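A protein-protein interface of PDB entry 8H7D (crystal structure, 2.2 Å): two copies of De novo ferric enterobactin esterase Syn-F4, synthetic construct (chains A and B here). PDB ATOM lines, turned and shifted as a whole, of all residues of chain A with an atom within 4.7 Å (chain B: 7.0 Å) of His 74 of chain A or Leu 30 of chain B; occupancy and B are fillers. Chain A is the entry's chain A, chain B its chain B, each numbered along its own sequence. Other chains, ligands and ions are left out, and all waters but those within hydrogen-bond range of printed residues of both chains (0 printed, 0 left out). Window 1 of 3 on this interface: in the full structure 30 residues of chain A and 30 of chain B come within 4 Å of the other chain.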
ATOM      1  N   ARG A  69      11.935  26.555 -16.026  1.00  0.00           N
ATOM      2  CA  ARG A  69      11.605  26.510 -14.590  1.00  0.00           C
ATOM      3  C   ARG A  69      12.627  25.702 -13.792  1.00  0.00           C
ATOM      4  O   ARG A  69      12.998  26.105 -12.700  1.00  0.00           O
ATOM      5  CB  ARG A  69      10.185  26.030 -14.356  1.00  0.00           C
ATOM      6  CG  ARG A  69       9.133  27.116 -14.620  1.00  0.00           C
ATOM      7  CD  ARG A  69       7.726  26.654 -14.260  1.00  0.00           C
ATOM      8  NE  ARG A  69       7.541  25.248 -14.621  1.00  0.00           N
ATOM      9  CZ  ARG A  69       7.299  24.785 -15.844  1.00  0.00           C
ATOM     10  NH1 ARG A  69       7.162  25.611 -16.872  1.00  0.00           N
ATOM     11  NH2 ARG A  69       7.165  23.473 -16.036  1.00  0.00           N
ATOM     12  N   ASP A  70      13.133  24.611 -14.362  1.00  0.00           N
ATOM     13  CA  ASP A  70      14.278  23.886 -13.753  1.00  0.00           C
ATOM     14  C   ASP A  70      15.370  24.899 -13.319  1.00  0.00           C
ATOM     15  O   ASP A  70      15.721  24.975 -12.131  1.00  0.00           O
ATOM     16  CB  ASP A  70      14.914  22.873 -14.723  1.00  0.00           C
ATOM     17  CG  ASP A  70      14.231  21.482 -14.737  1.00  0.00           C
ATOM     18  OD1 ASP A  70      13.314  21.203 -13.930  1.00  0.00           O
ATOM     19  OD2 ASP A  70      14.656  20.648 -15.592  1.00  0.00           O
ATOM     20  N   LEU A  71      15.852  25.706 -14.270  1.00  0.00           N
ATOM     21  CA  LEU A  71      16.863  26.740 -13.966  1.00  0.00           C
ATOM     22  C   LEU A  71      16.362  27.895 -13.080  1.00  0.00           C
ATOM     23  O   LEU A  71      17.078  28.351 -12.186  1.00  0.00           O
ATOM     24  CB  LEU A  71      17.478  27.318 -15.246  1.00  0.00           C
ATOM     25  CG  LEU A  71      18.571  28.377 -15.073  1.00  0.00           C
ATOM     26  CD1 LEU A  71      19.765  27.850 -14.292  1.00  0.00           C
ATOM     27  CD2 LEU A  71      19.020  28.874 -16.426  1.00  0.00           C
ATOM     28  N   ASP A  72      15.150  28.367 -13.342  1.00  0.00           N
ATOM     29  CA  ASP A  72      14.592  29.453 -12.581  1.00  0.00           C
ATOM     30  C   ASP A  72      14.506  29.097 -11.100  1.00  0.00           C
ATOM     31  O   ASP A  72      14.901  29.915 -10.234  1.00  0.00           O
ATOM     32  CB  ASP A  72      13.203  29.808 -13.116  1.00  0.00           C
ATOM     33  CG  ASP A  72      12.643  31.047 -12.477  1.00  0.00           C
ATOM     34  OD1 ASP A  72      13.404  32.001 -12.293  1.00  0.00           O
ATOM     35  OD2 ASP A  72      11.444  31.081 -12.154  1.00  0.00           O
ATOM     36  N   ASN A  73      13.990  27.884 -10.835  1.00  0.00           N
ATOM     37  CA  ASN A  73      13.973  27.271  -9.501  1.00  0.00           C
ATOM     38  C   ASN A  73      15.356  27.242  -8.882  1.00  0.00           C
ATOM     39  O   ASN A  73      15.580  27.816  -7.813  1.00  0.00           O
ATOM     40  CB  ASN A  73      13.428  25.830  -9.566  1.00  0.00           C
ATOM     41  CG  ASN A  73      13.285  25.190  -8.203  1.00  0.00           C
ATOM     42  OD1 ASN A  73      12.313  25.417  -7.534  1.00  0.00           O
ATOM     43  ND2 ASN A  73      14.289  24.426  -7.770  1.00  0.00           N
ATOM     44  N   HIS A  74      16.288  26.614  -9.582  1.00  0.00           N
ATOM     45  CA  HIS A  74      17.702  26.561  -9.132  1.00  0.00           C
ATOM     46  C   HIS A  74      18.244  27.944  -8.728  1.00  0.00           C
ATOM     47  O   HIS A  74      18.933  28.055  -7.728  1.00  0.00           O
ATOM     48  CB  HIS A  74      18.596  25.961 -10.195  1.00  0.00           C
ATOM     49  CG  HIS A  74      20.055  26.089  -9.872  1.00  0.00           C
ATOM     50  ND1 HIS A  74      20.651  25.385  -8.844  1.00  0.00           N
ATOM     51  CD2 HIS A  74      21.016  26.889 -10.390  1.00  0.00           C
ATOM     52  CE1 HIS A  74      21.916  25.744  -8.749  1.00  0.00           C
ATOM     53  NE2 HIS A  74      22.167  26.653  -9.677  1.00  0.00           N
ATOM     54  N   LEU A  75      17.894  28.988  -9.490  1.00  0.00           N
ATOM     55  CA  LEU A  75      18.461  30.311  -9.283  1.00  0.00           C
ATOM     56  C   LEU A  75      17.878  31.046  -8.080  1.00  0.00           C
ATOM     57  O   LEU A  75      18.608  31.691  -7.296  1.00  0.00           O
ATOM     58  CB  LEU A  75      18.319  31.143 -10.562  1.00  0.00           C
ATOM     59  CG  LEU A  75      19.315  30.781 -11.653  1.00  0.00           C
ATOM     60  CD1 LEU A  75      18.890  31.431 -12.953  1.00  0.00           C
ATOM     61  CD2 LEU A  75      20.763  31.168 -11.308  1.00  0.00           C
ATOM     62  N   GLN A  76      16.568  31.000  -7.957  1.00  0.00           N
ATOM     63  CA  GLN A  76      15.883  31.459  -6.717  1.00  0.00           C
ATOM     64  C   GLN A  76      16.401  30.733  -5.449  1.00  0.00           C
ATOM     65  O   GLN A  76      16.698  31.379  -4.439  1.00  0.00           O
ATOM     66  CB  GLN A  76      14.379  31.230  -6.832  1.00  0.00           C
ATOM     67  CG  GLN A  76      13.687  32.021  -7.927  1.00  0.00           C
ATOM     68  CD  GLN A  76      12.164  31.992  -7.773  1.00  0.00           C
ATOM     69  OE1 GLN A  76      11.627  32.505  -6.773  1.00  0.00           O
ATOM     70  NE2 GLN A  76      11.458  31.376  -8.745  1.00  0.00           N
ATOM     71  N   ARG A  77      16.490  29.398  -5.512  1.00  0.00           N
ATOM     72  CA  ARG A  77      17.062  28.572  -4.415  1.00  0.00           C
ATOM     73  C   ARG A  77      18.458  29.022  -4.041  1.00  0.00           C
ATOM     74  O   ARG A  77      18.761  29.200  -2.861  1.00  0.00           O
ATOM     75  CB  ARG A  77      17.144  27.095  -4.799  1.00  0.00           C
ATOM     76  CG  ARG A  77      15.790  26.392  -4.975  1.00  0.00           C
ATOM     77  CD  ARG A  77      15.227  25.829  -3.696  1.00  0.00           C
ATOM     78  NE  ARG A  77      16.010  24.700  -3.238  1.00  0.00           N
ATOM     79  CZ  ARG A  77      16.068  24.255  -1.977  1.00  0.00           C
ATOM     80  NH1 ARG A  77      15.371  24.852  -0.997  1.00  0.00           N
ATOM     81  NH2 ARG A  77      16.841  23.199  -1.683  1.00  0.00           N
ATOM     82  N   LYS A  78      19.300  29.190  -5.068  1.00  0.00           N
ATOM     83  CA  LYS A  78      20.674  29.659  -4.921  1.00  0.00           C
ATOM     84  C   LYS A  78      20.799  31.026  -4.238  1.00  0.00           C
ATOM     85  O   LYS A  78      21.688  31.241  -3.408  1.00  0.00           O
ATOM     86  CB  LYS A  78      21.320  29.709  -6.285  1.00  0.00           C
ATOM     87  CG  LYS A  78      22.799  30.029  -6.295  1.00  0.00           C
ATOM     88  CD  LYS A  78      23.721  28.836  -6.188  1.00  0.00           C
ATOM     89  CE  LYS A  78      25.155  29.321  -6.021  1.00  0.00           C
ATOM     90  NZ  LYS A  78      26.221  28.512  -6.651  1.00  0.00           N
ATOM     91  N   ASN B  22      26.187  21.587  -1.034  1.00  0.00           N
ATOM     92  CA  ASN B  22      25.493  22.408  -2.046  1.00  0.00           C
ATOM     93  C   ASN B  22      26.152  22.263  -3.416  1.00  0.00           C
ATOM     94  O   ASN B  22      25.471  22.016  -4.395  1.00  0.00           O
ATOM     95  CB  ASN B  22      25.413  23.883  -1.639  1.00  0.00           C
ATOM     96  CG  ASN B  22      24.516  24.113  -0.431  1.00  0.00           C
ATOM     97  OD1 ASN B  22      23.591  23.326  -0.159  1.00  0.00           O
ATOM     98  ND2 ASN B  22      24.790  25.197   0.318  1.00  0.00           N
ATOM     99  N   TRP B  23      27.477  22.336  -3.459  1.00  0.00           N
ATOM    100  CA  TRP B  23      28.172  22.125  -4.705  1.00  0.00           C
ATOM    101  C   TRP B  23      27.858  20.773  -5.359  1.00  0.00           C
ATOM    102  O   TRP B  23      27.632  20.718  -6.561  1.00  0.00           O
ATOM    103  CB  TRP B  23      29.678  22.311  -4.593  1.00  0.00           C
ATOM    104  CG  TRP B  23      30.304  21.936  -5.907  1.00  0.00           C
ATOM    105  CD1 TRP B  23      31.262  20.977  -6.126  1.00  0.00           C
ATOM    106  CD2 TRP B  23      29.929  22.429  -7.213  1.00  0.00           C
ATOM    107  NE1 TRP B  23      31.529  20.877  -7.476  1.00  0.00           N
ATOM    108  CE2 TRP B  23      30.735  21.761  -8.161  1.00  0.00           C
ATOM    109  CE3 TRP B  23      28.996  23.375  -7.672  1.00  0.00           C
ATOM    110  CZ2 TRP B  23      30.651  22.029  -9.533  1.00  0.00           C
ATOM    111  CZ3 TRP B  23      28.901  23.610  -9.041  1.00  0.00           C
ATOM    112  CH2 TRP B  23      29.724  22.944  -9.947  1.00  0.00           C
ATOM    113  N   ARG B  25      25.138  19.100  -5.117  1.00  0.00           N
ATOM    114  CA  ARG B  25      23.763  19.249  -5.605  1.00  0.00           C
ATOM    115  C   ARG B  25      23.660  20.125  -6.844  1.00  0.00           C
ATOM    116  O   ARG B  25      23.061  19.732  -7.860  1.00  0.00           O
ATOM    117  CB  ARG B  25      22.871  19.830  -4.501  1.00  0.00           C
ATOM    118  CG  ARG B  25      22.473  18.811  -3.429  1.00  0.00           C
ATOM    119  CD  ARG B  25      21.762  19.549  -2.305  1.00  0.00           C
ATOM    120  NE  ARG B  25      21.334  18.673  -1.227  1.00  0.00           N
ATOM    121  CZ  ARG B  25      21.078  19.065   0.027  1.00  0.00           C
ATOM    122  NH1 ARG B  25      21.144  20.338   0.393  1.00  0.00           N
ATOM    123  NH2 ARG B  25      20.734  18.164   0.928  1.00  0.00           N
ATOM    124  N   GLU B  26      24.237  21.317  -6.751  1.00  0.00           N
ATOM    125  CA  GLU B  26      24.301  22.223  -7.902  1.00  0.00           C
ATOM    126  C   GLU B  26      24.914  21.521  -9.127  1.00  0.00           C
ATOM    127  O   GLU B  26      24.310  21.489 -10.164  1.00  0.00           O
ATOM    128  CB  GLU B  26      25.095  23.484  -7.564  1.00  0.00           C
ATOM    129  CG  GLU B  26      25.251  24.437  -8.740  1.00  0.00           C
ATOM    130  CD  GLU B  26      25.601  25.856  -8.340  1.00  0.00           C
ATOM    131  OE1 GLU B  26      26.146  26.051  -7.223  1.00  0.00           O
ATOM    132  OE2 GLU B  26      25.317  26.775  -9.151  1.00  0.00           O
ATOM    133  N   ARG B  27      26.106  20.955  -8.965  1.00  0.00           N
ATOM    134  CA  ARG B  27      26.833  20.341 -10.041  1.00  0.00           C
ATOM    135  C   ARG B  27      25.981  19.306 -10.766  1.00  0.00           C
ATOM    136  O   ARG B  27      25.965  19.308 -11.982  1.00  0.00           O
ATOM    137  CB  ARG B  27      28.115  19.711  -9.534  1.00  0.00           C
ATOM    138  CG  ARG B  27      29.136  19.421 -10.625  1.00  0.00           C
ATOM    139  CD  ARG B  27      30.392  18.770 -10.034  1.00  0.00           C
ATOM    140  NE  ARG B  27      31.392  18.542 -11.073  1.00  0.00           N
ATOM    141  CZ  ARG B  27      31.390  17.513 -11.921  1.00  0.00           C
ATOM    142  NH1 ARG B  27      30.466  16.574 -11.854  1.00  0.00           N
ATOM    143  NH2 ARG B  27      32.338  17.403 -12.833  1.00  0.00           N
ATOM    144  N   ARG B  28      25.251  18.474 -10.022  1.00  0.00           N
ATOM    145  CA  ARG B  28      24.333  17.481 -10.592  1.00  0.00           C
ATOM    146  C   ARG B  28      23.151  18.113 -11.309  1.00  0.00           C
ATOM    147  O   ARG B  28      22.714  17.625 -12.368  1.00  0.00           O
ATOM    148  CB  ARG B  28      23.727  16.605  -9.500  1.00  0.00           C
ATOM    149  CG  ARG B  28      24.670  15.587  -8.879  1.00  0.00           C
ATOM    150  CD  ARG B  28      24.141  15.055  -7.537  1.00  0.00           C
ATOM    151  NE  ARG B  28      25.189  14.391  -6.749  1.00  0.00           N
ATOM    152  CZ  ARG B  28      25.147  14.152  -5.432  1.00  0.00           C
ATOM    153  NH1 ARG B  28      24.096  14.513  -4.688  1.00  0.00           N
ATOM    154  NH2 ARG B  28      26.181  13.540  -4.846  1.00  0.00           N
ATOM    155  N   THR B  29      22.571  19.130 -10.675  1.00  0.00           N
ATOM    156  CA  THR B  29      21.426  19.844 -11.239  1.00  0.00           C
ATOM    157  C   THR B  29      21.810  20.477 -12.597  1.00  0.00           C
ATOM    158  O   THR B  29      21.084  20.310 -13.575  1.00  0.00           O
ATOM    159  CB  THR B  29      20.894  20.920 -10.264  1.00  0.00           C
ATOM    160  OG1 THR B  29      20.523  20.313  -9.031  1.00  0.00           O
ATOM    161  CG2 THR B  29      19.682  21.680 -10.834  1.00  0.00           C
ATOM    162  N   LEU B  30      22.967  21.152 -12.640  1.00  0.00           N
ATOM    163  CA  LEU B  30      23.464  21.866 -13.851  1.00  0.00           C
ATOM    164  C   LEU B  30      23.978  20.944 -14.947  1.00  0.00           C
ATOM    165  O   LEU B  30      23.905  21.281 -16.121  1.00  0.00           O
ATOM    166  CB  LEU B  30      24.555  22.872 -13.454  1.00  0.00           C
ATOM    167  CG  LEU B  30      24.063  23.927 -12.433  1.00  0.00           C
ATOM    168  CD1 LEU B  30      25.160  24.897 -12.011  1.00  0.00           C
ATOM    169  CD2 LEU B  30      22.860  24.731 -12.938  1.00  0.00           C
ATOM    170  N   HIS B  31      24.506  19.791 -14.557  1.00  0.00           N
ATOM    171  CA  HIS B  31      25.027  18.787 -15.497  1.00  0.00           C
ATOM    172  C   HIS B  31      23.952  17.971 -16.181  1.00  0.00           C
ATOM    173  O   HIS B  31      24.097  17.669 -17.344  1.00  0.00           O
ATOM    174  CB  HIS B  31      26.025  17.851 -14.816  1.00  0.00           C
ATOM    175  CG  HIS B  31      27.414  18.369 -14.853  1.00  0.00           C
ATOM    176  ND1 HIS B  31      27.892  19.296 -13.949  1.00  0.00           N
ATOM    177  CD2 HIS B  31      28.419  18.131 -15.715  1.00  0.00           C
ATOM    178  CE1 HIS B  31      29.147  19.580 -14.231  1.00  0.00           C
ATOM    179  NE2 HIS B  31      29.491  18.885 -15.299  1.00  0.00           N
ATOM    180  N   ASP B  32      22.910  17.612 -15.435  1.00  0.00           N
ATOM    181  CA  ASP B  32      21.653  17.094 -15.975  1.00  0.00           C
ATOM    182  C   ASP B  32      20.964  18.109 -16.855  1.00  0.00           C
ATOM    183  O   ASP B  32      20.477  17.800 -17.967  1.00  0.00           O
ATOM    184  CB  ASP B  32      20.689  16.691 -14.840  1.00  0.00           C
ATOM    185  CG  ASP B  32      21.154  15.441 -14.090  1.00  0.00           C
ATOM    186  OD1 ASP B  32      22.171  14.848 -14.489  1.00  0.00           O
ATOM    187  OD2 ASP B  32      20.519  15.050 -13.097  1.00  0.00           O
ATOM    188  N   PHE B  33      20.932  19.325 -16.357  1.00  0.00           N
ATOM    189  CA  PHE B  33      20.413  20.440 -17.114  1.00  0.00           C
ATOM    190  C   PHE B  33      21.067  20.501 -18.499  1.00  0.00           C
ATOM    191  O   PHE B  33      20.378  20.422 -19.513  1.00  0.00           O
ATOM    192  CB  PHE B  33      20.607  21.763 -16.343  1.00  0.00           C
ATOM    193  CG  PHE B  33      19.908  22.915 -16.974  1.00  0.00           C
ATOM    194  CD1 PHE B  33      18.552  23.143 -16.740  1.00  0.00           C
ATOM    195  CD2 PHE B  33      20.583  23.739 -17.861  1.00  0.00           C
ATOM    196  CE1 PHE B  33      17.889  24.204 -17.373  1.00  0.00           C
ATOM    197  CE2 PHE B  33      19.936  24.797 -18.501  1.00  0.00           C
ATOM    198  CZ  PHE B  33      18.584  25.037 -18.254  1.00  0.00           C
ATOM    199  N   ALA B  34      22.393  20.614 -18.517  1.00  0.00           N
ATOM    200  CA  ALA B  34      23.172  20.660 -19.758  1.00  0.00           C
ATOM    201  C   ALA B  34      22.905  19.465 -20.679  1.00  0.00           C
ATOM    202  O   ALA B  34      22.700  19.642 -21.877  1.00  0.00           O
ATOM    203  CB  ALA B  34      24.648  20.694 -19.440  1.00  0.00           C
ATOM    204  N   ASP B  35      22.934  18.267 -20.109  1.00  0.00           N
ATOM    205  CA  ASP B  35      22.695  17.045 -20.860  1.00  0.00           C
ATOM    206  C   ASP B  35      21.345  17.067 -21.559  1.00  0.00           C
ATOM    207  O   ASP B  35      21.277  16.821 -22.753  1.00  0.00           O
ATOM    208  CB  ASP B  35      22.800  15.828 -19.952  1.00  0.00           C
ATOM    209  CG  ASP B  35      24.233  15.550 -19.500  1.00  0.00           C
ATOM    210  OD1 ASP B  35      25.203  15.909 -20.203  1.00  0.00           O
ATOM    211  OD2 ASP B  35      24.392  14.945 -18.427  1.00  0.00           O
ATOM    212  N   LEU B  71      26.818  27.308 -21.184  1.00  0.00           N
ATOM    213  CA  LEU B  71      26.675  26.517 -19.968  1.00  0.00           C
ATOM    214  C   LEU B  71      27.806  25.553 -19.785  1.00  0.00           C
ATOM    215  O   LEU B  71      28.450  25.532 -18.750  1.00  0.00           O
ATOM    216  CB  LEU B  71      25.356  25.745 -20.020  1.00  0.00           C
ATOM    217  CG  LEU B  71      24.997  24.871 -18.807  1.00  0.00           C
ATOM    218  CD1 LEU B  71      24.753  25.686 -17.536  1.00  0.00           C
ATOM    219  CD2 LEU B  71      23.783  24.012 -19.138  1.00  0.00           C
ATOM    220  N   HIS B  74      30.666  27.381 -18.766  1.00  0.00           N
ATOM    221  CA  HIS B  74      30.472  27.786 -17.363  1.00  0.00           C
ATOM    222  C   HIS B  74      30.780  26.684 -16.350  1.00  0.00           C
ATOM    223  O   HIS B  74      31.327  26.949 -15.284  1.00  0.00           O
ATOM    224  CB  HIS B  74      29.049  28.304 -17.125  1.00  0.00           C
ATOM    225  CG  HIS B  74      28.733  28.504 -15.680  1.00  0.00           C
ATOM    226  ND1 HIS B  74      29.290  29.520 -14.936  1.00  0.00           N
ATOM    227  CD2 HIS B  74      27.978  27.779 -14.823  1.00  0.00           C
ATOM    228  CE1 HIS B  74      28.886  29.419 -13.687  1.00  0.00           C
ATOM    229  NE2 HIS B  74      28.085  28.376 -13.592  1.00  0.00           N
ATOM    230  N   LEU B  75      30.433  25.445 -16.675  1.00  0.00           N
ATOM    231  CA  LEU B  75      30.610  24.332 -15.723  1.00  0.00           C
ATOM    232  C   LEU B  75      32.061  23.922 -15.625  1.00  0.00           C
ATOM    233  O   LEU B  75      32.539  23.605 -14.551  1.00  0.00           O
ATOM    234  CB  LEU B  75      29.757  23.138 -16.140  1.00  0.00           C
ATOM    235  CG  LEU B  75      28.261  23.423 -16.250  1.00  0.00           C
ATOM    236  CD1 LEU B  75      27.526  22.218 -16.816  1.00  0.00           C
ATOM    237  CD2 LEU B  75      27.665  23.899 -14.936  1.00  0.00           C
ATOM    238  N   LYS B  78      33.518  26.436 -13.455  1.00  0.00           N
ATOM    239  CA  LYS B  78      33.018  26.217 -12.093  1.00  0.00           C
ATOM    240  C   LYS B  78      33.822  25.103 -11.442  1.00  0.00           C
ATOM    241  O   LYS B  78      34.317  25.298 -10.349  1.00  0.00           O
ATOM    242  CB  LYS B  78      31.507  25.957 -12.061  1.00  0.00           C
ATOM    243  CG  LYS B  78      30.853  26.044 -10.696  1.00  0.00           C
ATOM    244  CD  LYS B  78      31.139  27.368  -9.976  1.00  0.00           C
ATOM    245  CE  LYS B  78      30.551  27.399  -8.575  1.00  0.00           C
ATOM    246  NZ  LYS B  78      29.103  27.133  -8.474  1.00  0.00           N
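Among the printed residues, pairs that only touch across the chains: Leu 71 of chain A with Phe 33 of chain B, His 74 of chain A with Leu 30 of chain B and Lys 78 of chain A with Lys 78 of chain B.
A ring nitrogen (NE2) of His 74 of chain A lies within hydrogen-bond range of the side-chain carboxylate (OE2) of Glu 26 of chain B, at 3.2 Å.
OE1 of Glu 26 of chain B lies within salt-bridge range of NZ of Lys 78 of chain A (2.5 Å).
NZ of Lys 78 of chain B is in salt-bridge range of OE1 of Glu 26 of chain B (3.4 Å).
His 74 of chain A touches just these residues of chain B: Glu 26 and Leu 30.
Of the printed residues of chain B, Lys 78 of chain A touches Glu 26 (2.5 Å) and Lys 78 (3.7 Å).
Printed residues of chain A within 4 Å of Lys 78 of chain B: Lys 78 (3.7 Å).
Of the printed residues of chain A, Glu 26 of chain B touches His 74 (3.2 Å) and Lys 78 (2.5 Å).
The nearest residue of chain A that does not touch Leu 30 of chain B is Leu 71 of chain A (4.6 Å).
Lys 78 of chain B touches its own counterpart, Lys 78 of chain A.
Of the 5 pairs that touch across the chains among the printed residues, 1 has its exchanged pair printed and touching as well.
Hydrophobic or aromatic side chains of chain B within 4 Å of the printed part of chain A: Leu 30 and Phe 33.
Of the 10 printed residues of chain A, 3 touch a printed residue of chain B.
Among the printed residues, 5 pairs touch across the chains.
Among the printed residues, Asp or Glu carboxylates within 4 Å of a Lys or Arg side-chain nitrogen of the other chain: Lys 78 of chain A with Glu 26 of chain B (2.5 Å).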
